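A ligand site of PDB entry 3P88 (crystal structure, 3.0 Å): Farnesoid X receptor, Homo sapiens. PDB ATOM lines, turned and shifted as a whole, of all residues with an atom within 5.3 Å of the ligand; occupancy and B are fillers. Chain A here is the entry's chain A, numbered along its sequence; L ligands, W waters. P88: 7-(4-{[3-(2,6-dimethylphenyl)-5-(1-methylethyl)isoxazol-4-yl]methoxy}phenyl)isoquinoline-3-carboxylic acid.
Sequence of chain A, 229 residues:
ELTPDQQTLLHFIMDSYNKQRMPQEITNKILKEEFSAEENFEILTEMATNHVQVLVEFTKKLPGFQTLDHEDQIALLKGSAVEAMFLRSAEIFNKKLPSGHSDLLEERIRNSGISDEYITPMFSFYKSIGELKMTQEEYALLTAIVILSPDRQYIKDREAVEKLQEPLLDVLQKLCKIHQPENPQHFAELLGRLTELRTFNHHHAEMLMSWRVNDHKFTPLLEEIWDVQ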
ATOM      1  N   MET A  22     -18.536  29.485   8.603  1.00  0.00           N
ATOM      2  CA  MET A  22     -17.640  30.488   9.150  1.00  0.00           C
ATOM      3  C   MET A  22     -16.846  31.111   8.008  1.00  0.00           C
ATOM      4  O   MET A  22     -16.195  30.396   7.249  1.00  0.00           O
ATOM      5  CB  MET A  22     -16.664  29.812  10.129  1.00  0.00           C
ATOM      6  CG  MET A  22     -15.935  30.761  11.050  1.00  0.00           C
ATOM      7  SD  MET A  22     -16.956  31.300  12.419  1.00  0.00           S
ATOM      8  CE  MET A  22     -17.207  29.758  13.279  1.00  0.00           C
ATOM      9  N   THR A  27     -11.594  33.848   9.931  1.00  0.00           N
ATOM     10  CA  THR A  27     -10.710  32.797  10.471  1.00  0.00           C
ATOM     11  C   THR A  27      -9.254  32.930  10.019  1.00  0.00           C
ATOM     12  O   THR A  27      -8.355  32.406  10.682  1.00  0.00           O
ATOM     13  CB  THR A  27     -11.219  31.384  10.126  1.00  0.00           C
ATOM     14  OG1 THR A  27     -11.412  31.257   8.709  1.00  0.00           O
ATOM     15  CG2 THR A  27     -12.526  31.078  10.843  1.00  0.00           C
ATOM     16  N   ILE A  30      -6.578  34.131  12.499  1.00  0.00           N
ATOM     17  CA  ILE A  30      -5.857  33.223  13.396  1.00  0.00           C
ATOM     18  C   ILE A  30      -4.400  33.124  12.950  1.00  0.00           C
ATOM     19  O   ILE A  30      -3.486  33.101  13.778  1.00  0.00           O
ATOM     20  CB  ILE A  30      -6.501  31.810  13.411  1.00  0.00           C
ATOM     21  CG1 ILE A  30      -7.906  31.872  14.010  1.00  0.00           C
ATOM     22  CG2 ILE A  30      -5.650  30.852  14.225  1.00  0.00           C
ATOM     23  CD1 ILE A  30      -8.679  30.580  13.892  1.00  0.00           C
ATOM     24  N   PHE A  41      -6.287  36.922  22.601  1.00  0.00           N
ATOM     25  CA  PHE A  41      -7.605  36.978  23.217  1.00  0.00           C
ATOM     26  C   PHE A  41      -8.646  37.646  22.318  1.00  0.00           C
ATOM     27  O   PHE A  41      -9.723  37.105  22.107  1.00  0.00           O
ATOM     28  CB  PHE A  41      -7.536  37.703  24.570  1.00  0.00           C
ATOM     29  CG  PHE A  41      -8.873  37.827  25.242  1.00  0.00           C
ATOM     30  CD1 PHE A  41      -9.623  38.985  25.100  1.00  0.00           C
ATOM     31  CD2 PHE A  41      -9.382  36.777  25.985  1.00  0.00           C
ATOM     32  CE1 PHE A  41     -10.861  39.085  25.695  1.00  0.00           C
ATOM     33  CE2 PHE A  41     -10.612  36.877  26.591  1.00  0.00           C
ATOM     34  CZ  PHE A  41     -11.362  38.035  26.449  1.00  0.00           C
ATOM     35  N   LEU A  44      -9.518  35.161  19.599  1.00  0.00           N
ATOM     36  CA  LEU A  44     -10.337  34.049  20.109  1.00  0.00           C
ATOM     37  C   LEU A  44     -11.779  34.470  20.391  1.00  0.00           C
ATOM     38  O   LEU A  44     -12.707  33.711  20.144  1.00  0.00           O
ATOM     39  CB  LEU A  44      -9.714  33.464  21.368  1.00  0.00           C
ATOM     40  CG  LEU A  44      -8.478  32.600  21.140  1.00  0.00           C
ATOM     41  CD1 LEU A  44      -7.806  32.275  22.470  1.00  0.00           C
ATOM     42  CD2 LEU A  44      -8.852  31.322  20.391  1.00  0.00           C
ATOM     43  N   THR A  45     -11.956  35.683  20.911  1.00  0.00           N
ATOM     44  CA  THR A  45     -13.285  36.230  21.141  1.00  0.00           C
ATOM     45  C   THR A  45     -14.024  36.440  19.822  1.00  0.00           C
ATOM     46  O   THR A  45     -15.207  36.127  19.712  1.00  0.00           O
ATOM     47  CB  THR A  45     -13.225  37.570  21.902  1.00  0.00           C
ATOM     48  OG1 THR A  45     -12.596  37.362  23.177  1.00  0.00           O
ATOM     49  CG2 THR A  45     -14.618  38.127  22.116  1.00  0.00           C
ATOM     50  N   MET A  47     -13.537  34.838  16.992  1.00  0.00           N
ATOM     51  CA  MET A  47     -13.874  33.501  16.501  1.00  0.00           C
ATOM     52  C   MET A  47     -15.134  32.963  17.175  1.00  0.00           C
ATOM     53  O   MET A  47     -16.045  32.471  16.505  1.00  0.00           O
ATOM     54  CB  MET A  47     -12.694  32.537  16.733  1.00  0.00           C
ATOM     55  CG  MET A  47     -11.846  32.251  15.495  1.00  0.00           C
ATOM     56  SD  MET A  47     -11.634  33.630  14.341  1.00  0.00           S
ATOM     57  CE  MET A  47     -10.688  34.785  15.328  1.00  0.00           C
ATOM     58  N   ALA A  48     -15.192  33.077  18.508  1.00  0.00           N
ATOM     59  CA  ALA A  48     -16.310  32.574  19.308  1.00  0.00           C
ATOM     60  C   ALA A  48     -17.664  33.178  18.911  1.00  0.00           C
ATOM     61  O   ALA A  48     -18.603  32.446  18.585  1.00  0.00           O
ATOM     62  CB  ALA A  48     -16.039  32.812  20.784  1.00  0.00           C
ATOM     63  N   HIS A  51     -18.803  32.093  15.681  1.00  0.00           N
ATOM     64  CA  HIS A  51     -19.237  30.703  15.800  1.00  0.00           C
ATOM     65  C   HIS A  51     -20.601  30.574  16.490  1.00  0.00           C
ATOM     66  O   HIS A  51     -21.392  29.700  16.130  1.00  0.00           O
ATOM     67  CB  HIS A  51     -18.185  29.850  16.510  1.00  0.00           C
ATOM     68  CG  HIS A  51     -18.458  28.383  16.422  1.00  0.00           C
ATOM     69  ND1 HIS A  51     -18.316  27.527  17.497  1.00  0.00           N
ATOM     70  CD2 HIS A  51     -18.902  27.619  15.399  1.00  0.00           C
ATOM     71  CE1 HIS A  51     -18.634  26.299  17.124  1.00  0.00           C
ATOM     72  NE2 HIS A  51     -18.992  26.328  15.857  1.00  0.00           N
ATOM     73  N   VAL A  82     -21.158  26.544  25.100  1.00  0.00           N
ATOM     74  CA  VAL A  82     -19.748  26.208  25.288  1.00  0.00           C
ATOM     75  C   VAL A  82     -19.434  24.806  24.810  1.00  0.00           C
ATOM     76  O   VAL A  82     -18.411  24.587  24.157  1.00  0.00           O
ATOM     77  CB  VAL A  82     -19.338  26.308  26.778  1.00  0.00           C
ATOM     78  CG1 VAL A  82     -18.003  25.645  27.007  1.00  0.00           C
ATOM     79  CG2 VAL A  82     -19.295  27.754  27.215  1.00  0.00           C
ATOM     80  N   MET A  85     -19.180  24.542  21.108  1.00  0.00           N
ATOM     81  CA  MET A  85     -17.947  25.225  20.729  1.00  0.00           C
ATOM     82  C   MET A  85     -16.733  24.354  21.007  1.00  0.00           C
ATOM     83  O   MET A  85     -15.817  24.276  20.197  1.00  0.00           O
ATOM     84  CB  MET A  85     -17.811  26.568  21.454  1.00  0.00           C
ATOM     85  CG  MET A  85     -18.563  27.705  20.788  1.00  0.00           C
ATOM     86  SD  MET A  85     -18.500  29.239  21.720  1.00  0.00           S
ATOM     87  CE  MET A  85     -20.104  29.228  22.491  1.00  0.00           C
ATOM     88  N   PHE A  86     -16.736  23.712  22.176  1.00  0.00           N
ATOM     89  CA  PHE A  86     -15.657  22.812  22.581  1.00  0.00           C
ATOM     90  C   PHE A  86     -15.555  21.635  21.624  1.00  0.00           C
ATOM     91  O   PHE A  86     -14.470  21.123  21.339  1.00  0.00           O
ATOM     92  CB  PHE A  86     -15.900  22.285  23.996  1.00  0.00           C
ATOM     93  CG  PHE A  86     -14.791  22.577  24.949  1.00  0.00           C
ATOM     94  CD1 PHE A  86     -14.929  23.572  25.922  1.00  0.00           C
ATOM     95  CD2 PHE A  86     -13.606  21.853  24.895  1.00  0.00           C
ATOM     96  CE1 PHE A  86     -13.897  23.845  26.818  1.00  0.00           C
ATOM     97  CE2 PHE A  86     -12.568  22.119  25.786  1.00  0.00           C
ATOM     98  CZ  PHE A  86     -12.720  23.121  26.752  1.00  0.00           C
ATOM     99  N   ARG A  88     -16.550  21.617  18.396  1.00  0.00           N
ATOM    100  CA  ARG A  88     -16.098  22.085  17.069  1.00  0.00           C
ATOM    101  C   ARG A  88     -14.600  22.364  17.054  1.00  0.00           C
ATOM    102  O   ARG A  88     -13.919  22.031  16.087  1.00  0.00           O
ATOM    103  CB  ARG A  88     -16.855  23.351  16.640  1.00  0.00           C
ATOM    104  CG  ARG A  88     -17.390  23.305  15.212  1.00  0.00           C
ATOM    105  CD  ARG A  88     -16.308  23.247  14.149  1.00  0.00           C
ATOM    106  NE  ARG A  88     -16.889  22.892  12.844  1.00  0.00           N
ATOM    107  CZ  ARG A  88     -16.223  22.881  11.692  1.00  0.00           C
ATOM    108  NH1 ARG A  88     -14.945  23.212  11.633  1.00  0.00           N
ATOM    109  NH2 ARG A  88     -16.852  22.529  10.569  1.00  0.00           N
ATOM    110  N   SER A  89     -14.101  22.986  18.116  1.00  0.00           N
ATOM    111  CA  SER A  89     -12.668  23.262  18.267  1.00  0.00           C
ATOM    112  C   SER A  89     -11.859  21.982  18.401  1.00  0.00           C
ATOM    113  O   SER A  89     -10.691  21.939  18.011  1.00  0.00           O
ATOM    114  CB  SER A  89     -12.411  24.149  19.481  1.00  0.00           C
ATOM    115  OG  SER A  89     -12.525  23.426  20.684  1.00  0.00           O
ATOM    116  N   ILE A  92     -11.282  20.813  15.002  1.00  0.00           N
ATOM    117  CA  ILE A  92     -10.209  21.591  14.391  1.00  0.00           C
ATOM    118  C   ILE A  92      -8.875  20.894  14.647  1.00  0.00           C
ATOM    119  O   ILE A  92      -8.163  20.554  13.710  1.00  0.00           O
ATOM    120  CB  ILE A  92     -10.113  23.039  14.947  1.00  0.00           C
ATOM    121  CG1 ILE A  92     -11.366  23.857  14.601  1.00  0.00           C
ATOM    122  CG2 ILE A  92      -8.884  23.749  14.407  1.00  0.00           C
ATOM    123  CD1 ILE A  92     -11.641  23.984  13.122  1.00  0.00           C
ATOM    124  N   SER A  99      -9.048  25.748   7.438  1.00  0.00           N
ATOM    125  CA  SER A  99      -9.643  27.037   7.827  1.00  0.00           C
ATOM    126  C   SER A  99      -9.667  27.273   9.344  1.00  0.00           C
ATOM    127  O   SER A  99      -9.982  28.378   9.786  1.00  0.00           O
ATOM    128  CB  SER A  99     -11.055  27.155   7.250  1.00  0.00           C
ATOM    129  N   GLY A 100      -9.344  26.243  10.137  1.00  0.00           N
ATOM    130  CA  GLY A 100      -9.256  26.368  11.592  1.00  0.00           C
ATOM    131  C   GLY A 100      -7.876  26.753  12.100  1.00  0.00           C
ATOM    132  O   GLY A 100      -7.750  27.337  13.171  1.00  0.00           O
ATOM    133  N   LEU A 105      -4.045  28.415  16.174  1.00  0.00           N
ATOM    134  CA  LEU A 105      -5.156  28.499  17.112  1.00  0.00           C
ATOM    135  C   LEU A 105      -4.715  28.011  18.498  1.00  0.00           C
ATOM    136  O   LEU A 105      -5.085  28.587  19.517  1.00  0.00           O
ATOM    137  CB  LEU A 105      -6.354  27.669  16.612  1.00  0.00           C
ATOM    138  CG  LEU A 105      -7.668  27.785  17.397  1.00  0.00           C
ATOM    139  CD1 LEU A 105      -8.240  29.187  17.323  1.00  0.00           C
ATOM    140  CD2 LEU A 105      -8.683  26.776  16.873  1.00  0.00           C
ATOM    141  N   ILE A 109      -4.657  30.134  22.099  1.00  0.00           N
ATOM    142  CA  ILE A 109      -5.333  29.596  23.280  1.00  0.00           C
ATOM    143  C   ILE A 109      -4.338  29.461  24.439  1.00  0.00           C
ATOM    144  O   ILE A 109      -4.634  29.881  25.570  1.00  0.00           O
ATOM    145  CB  ILE A 109      -5.976  28.226  23.002  1.00  0.00           C
ATOM    146  CG1 ILE A 109      -7.185  28.385  22.079  1.00  0.00           C
ATOM    147  CG2 ILE A 109      -6.412  27.564  24.300  1.00  0.00           C
ATOM    148  CD1 ILE A 109      -7.735  27.082  21.556  1.00  0.00           C
ATOM    149  N   ILE A 114      -5.442  32.213  30.110  1.00  0.00           N
ATOM    150  CA  ILE A 114      -6.045  30.998  30.667  1.00  0.00           C
ATOM    151  C   ILE A 114      -5.052  30.265  31.573  1.00  0.00           C
ATOM    152  O   ILE A 114      -3.884  30.102  31.225  1.00  0.00           O
ATOM    153  CB  ILE A 114      -6.508  30.012  29.561  1.00  0.00           C
ATOM    154  CG1 ILE A 114      -7.489  30.683  28.603  1.00  0.00           C
ATOM    155  CG2 ILE A 114      -7.185  28.795  30.178  1.00  0.00           C
ATOM    156  CD1 ILE A 114      -7.735  29.874  27.356  1.00  0.00           C
ATOM    157  N   MET A 122      -8.216  20.704  29.208  1.00  0.00           N
ATOM    158  CA  MET A 122      -8.764  21.102  27.922  1.00  0.00           C
ATOM    159  C   MET A 122      -8.074  20.398  26.765  1.00  0.00           C
ATOM    160  O   MET A 122      -8.726  19.952  25.820  1.00  0.00           O
ATOM    161  CB  MET A 122      -8.634  22.615  27.782  1.00  0.00           C
ATOM    162  CG  MET A 122      -9.050  23.185  26.448  1.00  0.00           C
ATOM    163  SD  MET A 122      -9.039  24.979  26.478  1.00  0.00           S
ATOM    164  CE  MET A 122      -9.991  25.309  27.961  1.00  0.00           C
ATOM    165  N   TYR A 126      -8.774  17.109  24.144  1.00  0.00           N
ATOM    166  CA  TYR A 126      -8.556  17.149  22.692  1.00  0.00           C
ATOM    167  C   TYR A 126      -7.778  15.933  22.203  1.00  0.00           C
ATOM    168  O   TYR A 126      -8.121  15.336  21.188  1.00  0.00           O
ATOM    169  CB  TYR A 126      -7.828  18.436  22.273  1.00  0.00           C
ATOM    170  CG  TYR A 126      -8.620  19.718  22.437  1.00  0.00           C
ATOM    171  CD1 TYR A 126      -9.956  19.799  22.048  1.00  0.00           C
ATOM    172  CD2 TYR A 126      -8.015  20.869  22.920  1.00  0.00           C
ATOM    173  CE1 TYR A 126     -10.673  20.986  22.185  1.00  0.00           C
ATOM    174  CE2 TYR A 126      -8.718  22.055  23.056  1.00  0.00           C
ATOM    175  CZ  TYR A 126     -10.039  22.119  22.692  1.00  0.00           C
ATOM    176  OH  TYR A 126     -10.728  23.298  22.835  1.00  0.00           O
ATOM    177  N   HIS A 204     -15.348  26.469  32.394  1.00  0.00           N
ATOM    178  CA  HIS A 204     -15.537  27.668  31.586  1.00  0.00           C
ATOM    179  C   HIS A 204     -16.032  28.871  32.404  1.00  0.00           C
ATOM    180  O   HIS A 204     -15.609  30.007  32.170  1.00  0.00           O
ATOM    181  CB  HIS A 204     -16.499  27.371  30.435  1.00  0.00           C
ATOM    182  CG  HIS A 204     -16.520  28.427  29.390  1.00  0.00           C
ATOM    183  ND1 HIS A 204     -17.468  29.422  29.350  1.00  0.00           N
ATOM    184  CD2 HIS A 204     -15.689  28.657  28.340  1.00  0.00           C
ATOM    185  CE1 HIS A 204     -17.227  30.213  28.318  1.00  0.00           C
ATOM    186  NE2 HIS A 204     -16.156  29.772  27.700  1.00  0.00           N
ATOM    187  N   LEU A 208     -14.052  32.455  32.448  1.00  0.00           N
ATOM    188  CA  LEU A 208     -14.631  33.758  32.146  1.00  0.00           C
ATOM    189  C   LEU A 208     -14.415  34.727  33.294  1.00  0.00           C
ATOM    190  O   LEU A 208     -14.095  35.896  33.072  1.00  0.00           O
ATOM    191  CB  LEU A 208     -16.127  33.654  31.833  1.00  0.00           C
ATOM    192  CG  LEU A 208     -16.545  32.966  30.525  1.00  0.00           C
ATOM    193  CD1 LEU A 208     -18.020  33.188  30.278  1.00  0.00           C
ATOM    194  CD2 LEU A 208     -15.739  33.457  29.322  1.00  0.00           C
ATOM    195  N   TRP A 211     -10.844  36.273  33.217  1.00  0.00           N
ATOM    196  CA  TRP A 211     -10.703  37.305  32.187  1.00  0.00           C
ATOM    197  C   TRP A 211     -11.364  38.607  32.622  1.00  0.00           C
ATOM    198  O   TRP A 211     -10.807  39.687  32.432  1.00  0.00           O
ATOM    199  CB  TRP A 211     -11.308  36.842  30.873  1.00  0.00           C
ATOM    200  CG  TRP A 211     -10.443  35.922  30.084  1.00  0.00           C
ATOM    201  CD1 TRP A 211      -9.128  36.092  29.791  1.00  0.00           C
ATOM    202  CD2 TRP A 211     -10.845  34.711  29.451  1.00  0.00           C
ATOM    203  NE1 TRP A 211      -8.679  35.040  29.023  1.00  0.00           N
ATOM    204  CE2 TRP A 211      -9.714  34.182  28.798  1.00  0.00           C
ATOM    205  CE3 TRP A 211     -12.060  34.014  29.369  1.00  0.00           C
ATOM    206  CZ2 TRP A 211      -9.757  33.000  28.078  1.00  0.00           C
ATOM    207  CZ3 TRP A 211     -12.103  32.832  28.650  1.00  0.00           C
ATOM    208  CH2 TRP A 211     -10.953  32.337  28.018  1.00  0.00           C
ATOM    209  N   PHE A 218     -15.950  41.019  26.423  1.00  0.00           N
ATOM    210  CA  PHE A 218     -16.396  39.994  25.494  1.00  0.00           C
ATOM    211  C   PHE A 218     -17.267  40.655  24.408  1.00  0.00           C
ATOM    212  O   PHE A 218     -16.832  41.638  23.802  1.00  0.00           O
ATOM    213  CB  PHE A 218     -17.104  38.856  26.245  1.00  0.00           C
ATOM    214  CG  PHE A 218     -16.211  38.135  27.221  1.00  0.00           C
ATOM    215  CD1 PHE A 218     -16.376  38.294  28.586  1.00  0.00           C
ATOM    216  CD2 PHE A 218     -15.197  37.301  26.768  1.00  0.00           C
ATOM    217  CE1 PHE A 218     -15.542  37.632  29.482  1.00  0.00           C
ATOM    218  CE2 PHE A 218     -14.370  36.639  27.653  1.00  0.00           C
ATOM    219  CZ  PHE A 218     -14.542  36.810  29.014  1.00  0.00           C
ATOM    220  N   LEU A 222     -22.058  36.945  23.157  1.00  0.00           N
ATOM    221  CA  LEU A 222     -21.460  35.991  24.086  1.00  0.00           C
ATOM    222  C   LEU A 222     -21.895  36.264  25.519  1.00  0.00           C
ATOM    223  O   LEU A 222     -22.199  35.336  26.275  1.00  0.00           O
ATOM    224  CB  LEU A 222     -19.934  36.068  24.025  1.00  0.00           C
ATOM    225  CG  LEU A 222     -19.279  35.440  22.798  1.00  0.00           C
ATOM    226  CD1 LEU A 222     -17.813  35.812  22.737  1.00  0.00           C
ATOM    227  CD2 LEU A 222     -19.460  33.936  22.827  1.00  0.00           C
ATOM    228  N   TRP A 226     -23.792  33.306  27.618  1.00  0.00           N
ATOM    229  CA  TRP A 226     -23.140  32.785  28.823  1.00  0.00           C
ATOM    230  C   TRP A 226     -23.563  33.479  30.121  1.00  0.00           C
ATOM    231  O   TRP A 226     -23.247  32.985  31.199  1.00  0.00           O
ATOM    232  CB  TRP A 226     -21.611  32.881  28.691  1.00  0.00           C
ATOM    233  CG  TRP A 226     -21.036  32.023  27.604  1.00  0.00           C
ATOM    234  CD1 TRP A 226     -21.522  30.828  27.149  1.00  0.00           C
ATOM    235  CD2 TRP A 226     -19.850  32.284  26.850  1.00  0.00           C
ATOM    236  NE1 TRP A 226     -20.722  30.338  26.150  1.00  0.00           N
ATOM    237  CE2 TRP A 226     -19.686  31.203  25.953  1.00  0.00           C
ATOM    238  CE3 TRP A 226     -18.905  33.318  26.846  1.00  0.00           C
ATOM    239  CZ2 TRP A 226     -18.612  31.136  25.050  1.00  0.00           C
ATOM    240  CZ3 TRP A 226     -17.845  33.247  25.953  1.00  0.00           C
ATOM    241  CH2 TRP A 226     -17.708  32.163  25.066  1.00  0.00           C
HETATM  242  C1  P88 L   1     -11.882  34.021  24.370  1.00  0.00           C
HETATM  243  N1  P88 L   1     -13.783  30.276  25.716  1.00  0.00           N
HETATM  244  O1  P88 L   1     -13.746  31.699  25.581  1.00  0.00           O
HETATM  245  C2  P88 L   1     -13.250  33.484  23.991  1.00  0.00           C
HETATM  246  N2  P88 L   1     -15.539  26.853  12.090  1.00  0.00           N
HETATM  247  O2  P88 L   1     -13.588  29.795  21.521  1.00  0.00           O
HETATM  248  C3  P88 L   1     -14.362  34.258  24.693  1.00  0.00           C
HETATM  249  O3  P88 L   1     -13.340  26.759   9.242  1.00  0.00           O
HETATM  250  C4  P88 L   1     -13.348  32.048  24.333  1.00  0.00           C
HETATM  251  O4  P88 L   1     -15.439  26.155   9.397  1.00  0.00           O
HETATM  252  C5  P88 L   1     -13.386  29.741  24.533  1.00  0.00           C
HETATM  253  C6  P88 L   1     -13.106  30.779  23.622  1.00  0.00           C
HETATM  254  C7  P88 L   1     -12.640  30.626  22.194  1.00  0.00           C
HETATM  255  C8  P88 L   1     -13.506  29.476  20.186  1.00  0.00           C
HETATM  256  C9  P88 L   1     -14.639  29.016  19.542  1.00  0.00           C
HETATM  257  C10 P88 L   1     -14.603  28.677  18.196  1.00  0.00           C
HETATM  258  C11 P88 L   1     -13.430  28.784  17.450  1.00  0.00           C
HETATM  259  C12 P88 L   1     -12.286  29.255  18.113  1.00  0.00           C
HETATM  260  C13 P88 L   1     -12.323  29.594  19.459  1.00  0.00           C
HETATM  261  C14 P88 L   1     -13.395  28.444  16.079  1.00  0.00           C
HETATM  262  C15 P88 L   1     -12.198  28.566  15.343  1.00  0.00           C
HETATM  263  C16 P88 L   1     -12.148  28.231  13.988  1.00  0.00           C
HETATM  264  C17 P88 L   1     -13.275  27.765  13.339  1.00  0.00           C
HETATM  265  C18 P88 L   1     -13.239  27.426  11.993  1.00  0.00           C
HETATM  266  C19 P88 L   1     -14.392  26.963  11.370  1.00  0.00           C
HETATM  267  C20 P88 L   1     -15.596  27.174  13.389  1.00  0.00           C
HETATM  268  C21 P88 L   1     -14.468  27.635  14.046  1.00  0.00           C
HETATM  269  C22 P88 L   1     -14.519  27.975  15.393  1.00  0.00           C
HETATM  270  C23 P88 L   1     -14.381  26.597   9.913  1.00  0.00           C
HETATM  271  C24 P88 L   1     -13.270  28.283  24.226  1.00  0.00           C
HETATM  272  C25 P88 L   1     -14.409  27.538  24.004  1.00  0.00           C
HETATM  273  C26 P88 L   1     -14.332  26.187  23.709  1.00  0.00           C
HETATM  274  C27 P88 L   1     -13.082  25.568  23.636  1.00  0.00           C
HETATM  275  C28 P88 L   1     -11.930  26.312  23.856  1.00  0.00           C
HETATM  276  C29 P88 L   1     -12.027  27.675  24.149  1.00  0.00           C
HETATM  277  CL1 P88 L   1     -16.020  28.322  24.097  1.00  0.00           C
HETATM  278  CL2 P88 L   1     -10.525  28.596  24.438  1.00  0.00           C
HETATM  279  O   HOH W   1     -17.414  26.969   7.202  1.00  0.00           O
HETATM  280  O   HOH W   2     -13.127  29.489   7.942  1.00  0.00           O
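A ring nitrogen (NE2) of His 204 is in hydrogen-bond range of a nitrogen (N1) of the ligand. The guanidinium group (NH1) of Arg 88 lies within salt-bridge range of an oxygen (O4) of the ligand, 3.7 Å away.
The backbone carbonyl oxygen (O) of Phe 86 is in hydrogen-bond range of the side-chain hydroxyl (OG) of Ser 89 (3.1 Å). The side-chain hydroxyl of Ser 89 is in hydrogen-bond range of the backbone carbonyl oxygen of Met 85 (3.4 Å). The side-chain hydroxyl (OG1) of Thr 45 is in hydrogen-bond range of the backbone carbonyl oxygen (O) of Phe 41, 3.1 Å away. OG of Ser 89 is in hydrogen-bond range of OH of Tyr 126 (2.8 Å). OG1 of Thr 27 lies close to O of Ser 99, 3.4 Å away.
Met 22 touches the ligand. CG2 of Thr 27 touches C18 of the ligand, at 3.9 Å. CE2 of Phe 41 touches C1 of the ligand, at 3.8 Å. Leu 44 touches the ligand (O to C7, 3.7 Å). OG1 of Thr 45 touches C1 of the ligand, at 3.6 Å. CB of Met 47 touches C12 of the ligand, at 3.6 Å. Ala 48 touches the ligand (CA to C9, 3.9 Å). CD2 of His 51 touches C20 of the ligand, 3.9 Å away. SD of Met 85 touches CL1 of the ligand (3.6 Å). Phe 86 touches the ligand. Ser 89 touches the ligand. CD1 of Ile 92 touches C18 of the ligand (3.96 Å). Ser 99 touches the ligand. Tyr 126 touches the ligand. Trp 211 touches the ligand. Phe 218 touches the ligand (CD2 to C3, 3.8 Å). Trp 226 touches the ligand. Hydrophobic or aromatic side chains within 4 Å of the ligand: Met 22, Phe 41, Leu 44, Met 47, Ala 48, His 51, Met 85, Phe 86, Ile 92, His 204, Trp 211, Phe 218 and Trp 226. Within 4 Å of the ligand: Met 22, Thr 27, Phe 41, Leu 44, Thr 45, Met 47, Ala 48, His 51, Met 85, Phe 86, Arg 88, Ser 89, Ile 92, Ser 99, Tyr 126, His 204, Trp 211, Phe 218 and Trp 226.
Water W2 lies within hydrogen-bond range of the side-chain hydroxyl (OG1) of Thr 27 (2.6 Å), an oxygen (O3) of the ligand (3.0 Å) and the backbone carbonyl oxygen (O) of Met 22 (3.3 Å). Water W1 lies within hydrogen-bond range of O4 of the ligand (3.1 Å) and N of Met 22 (3.1 Å).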
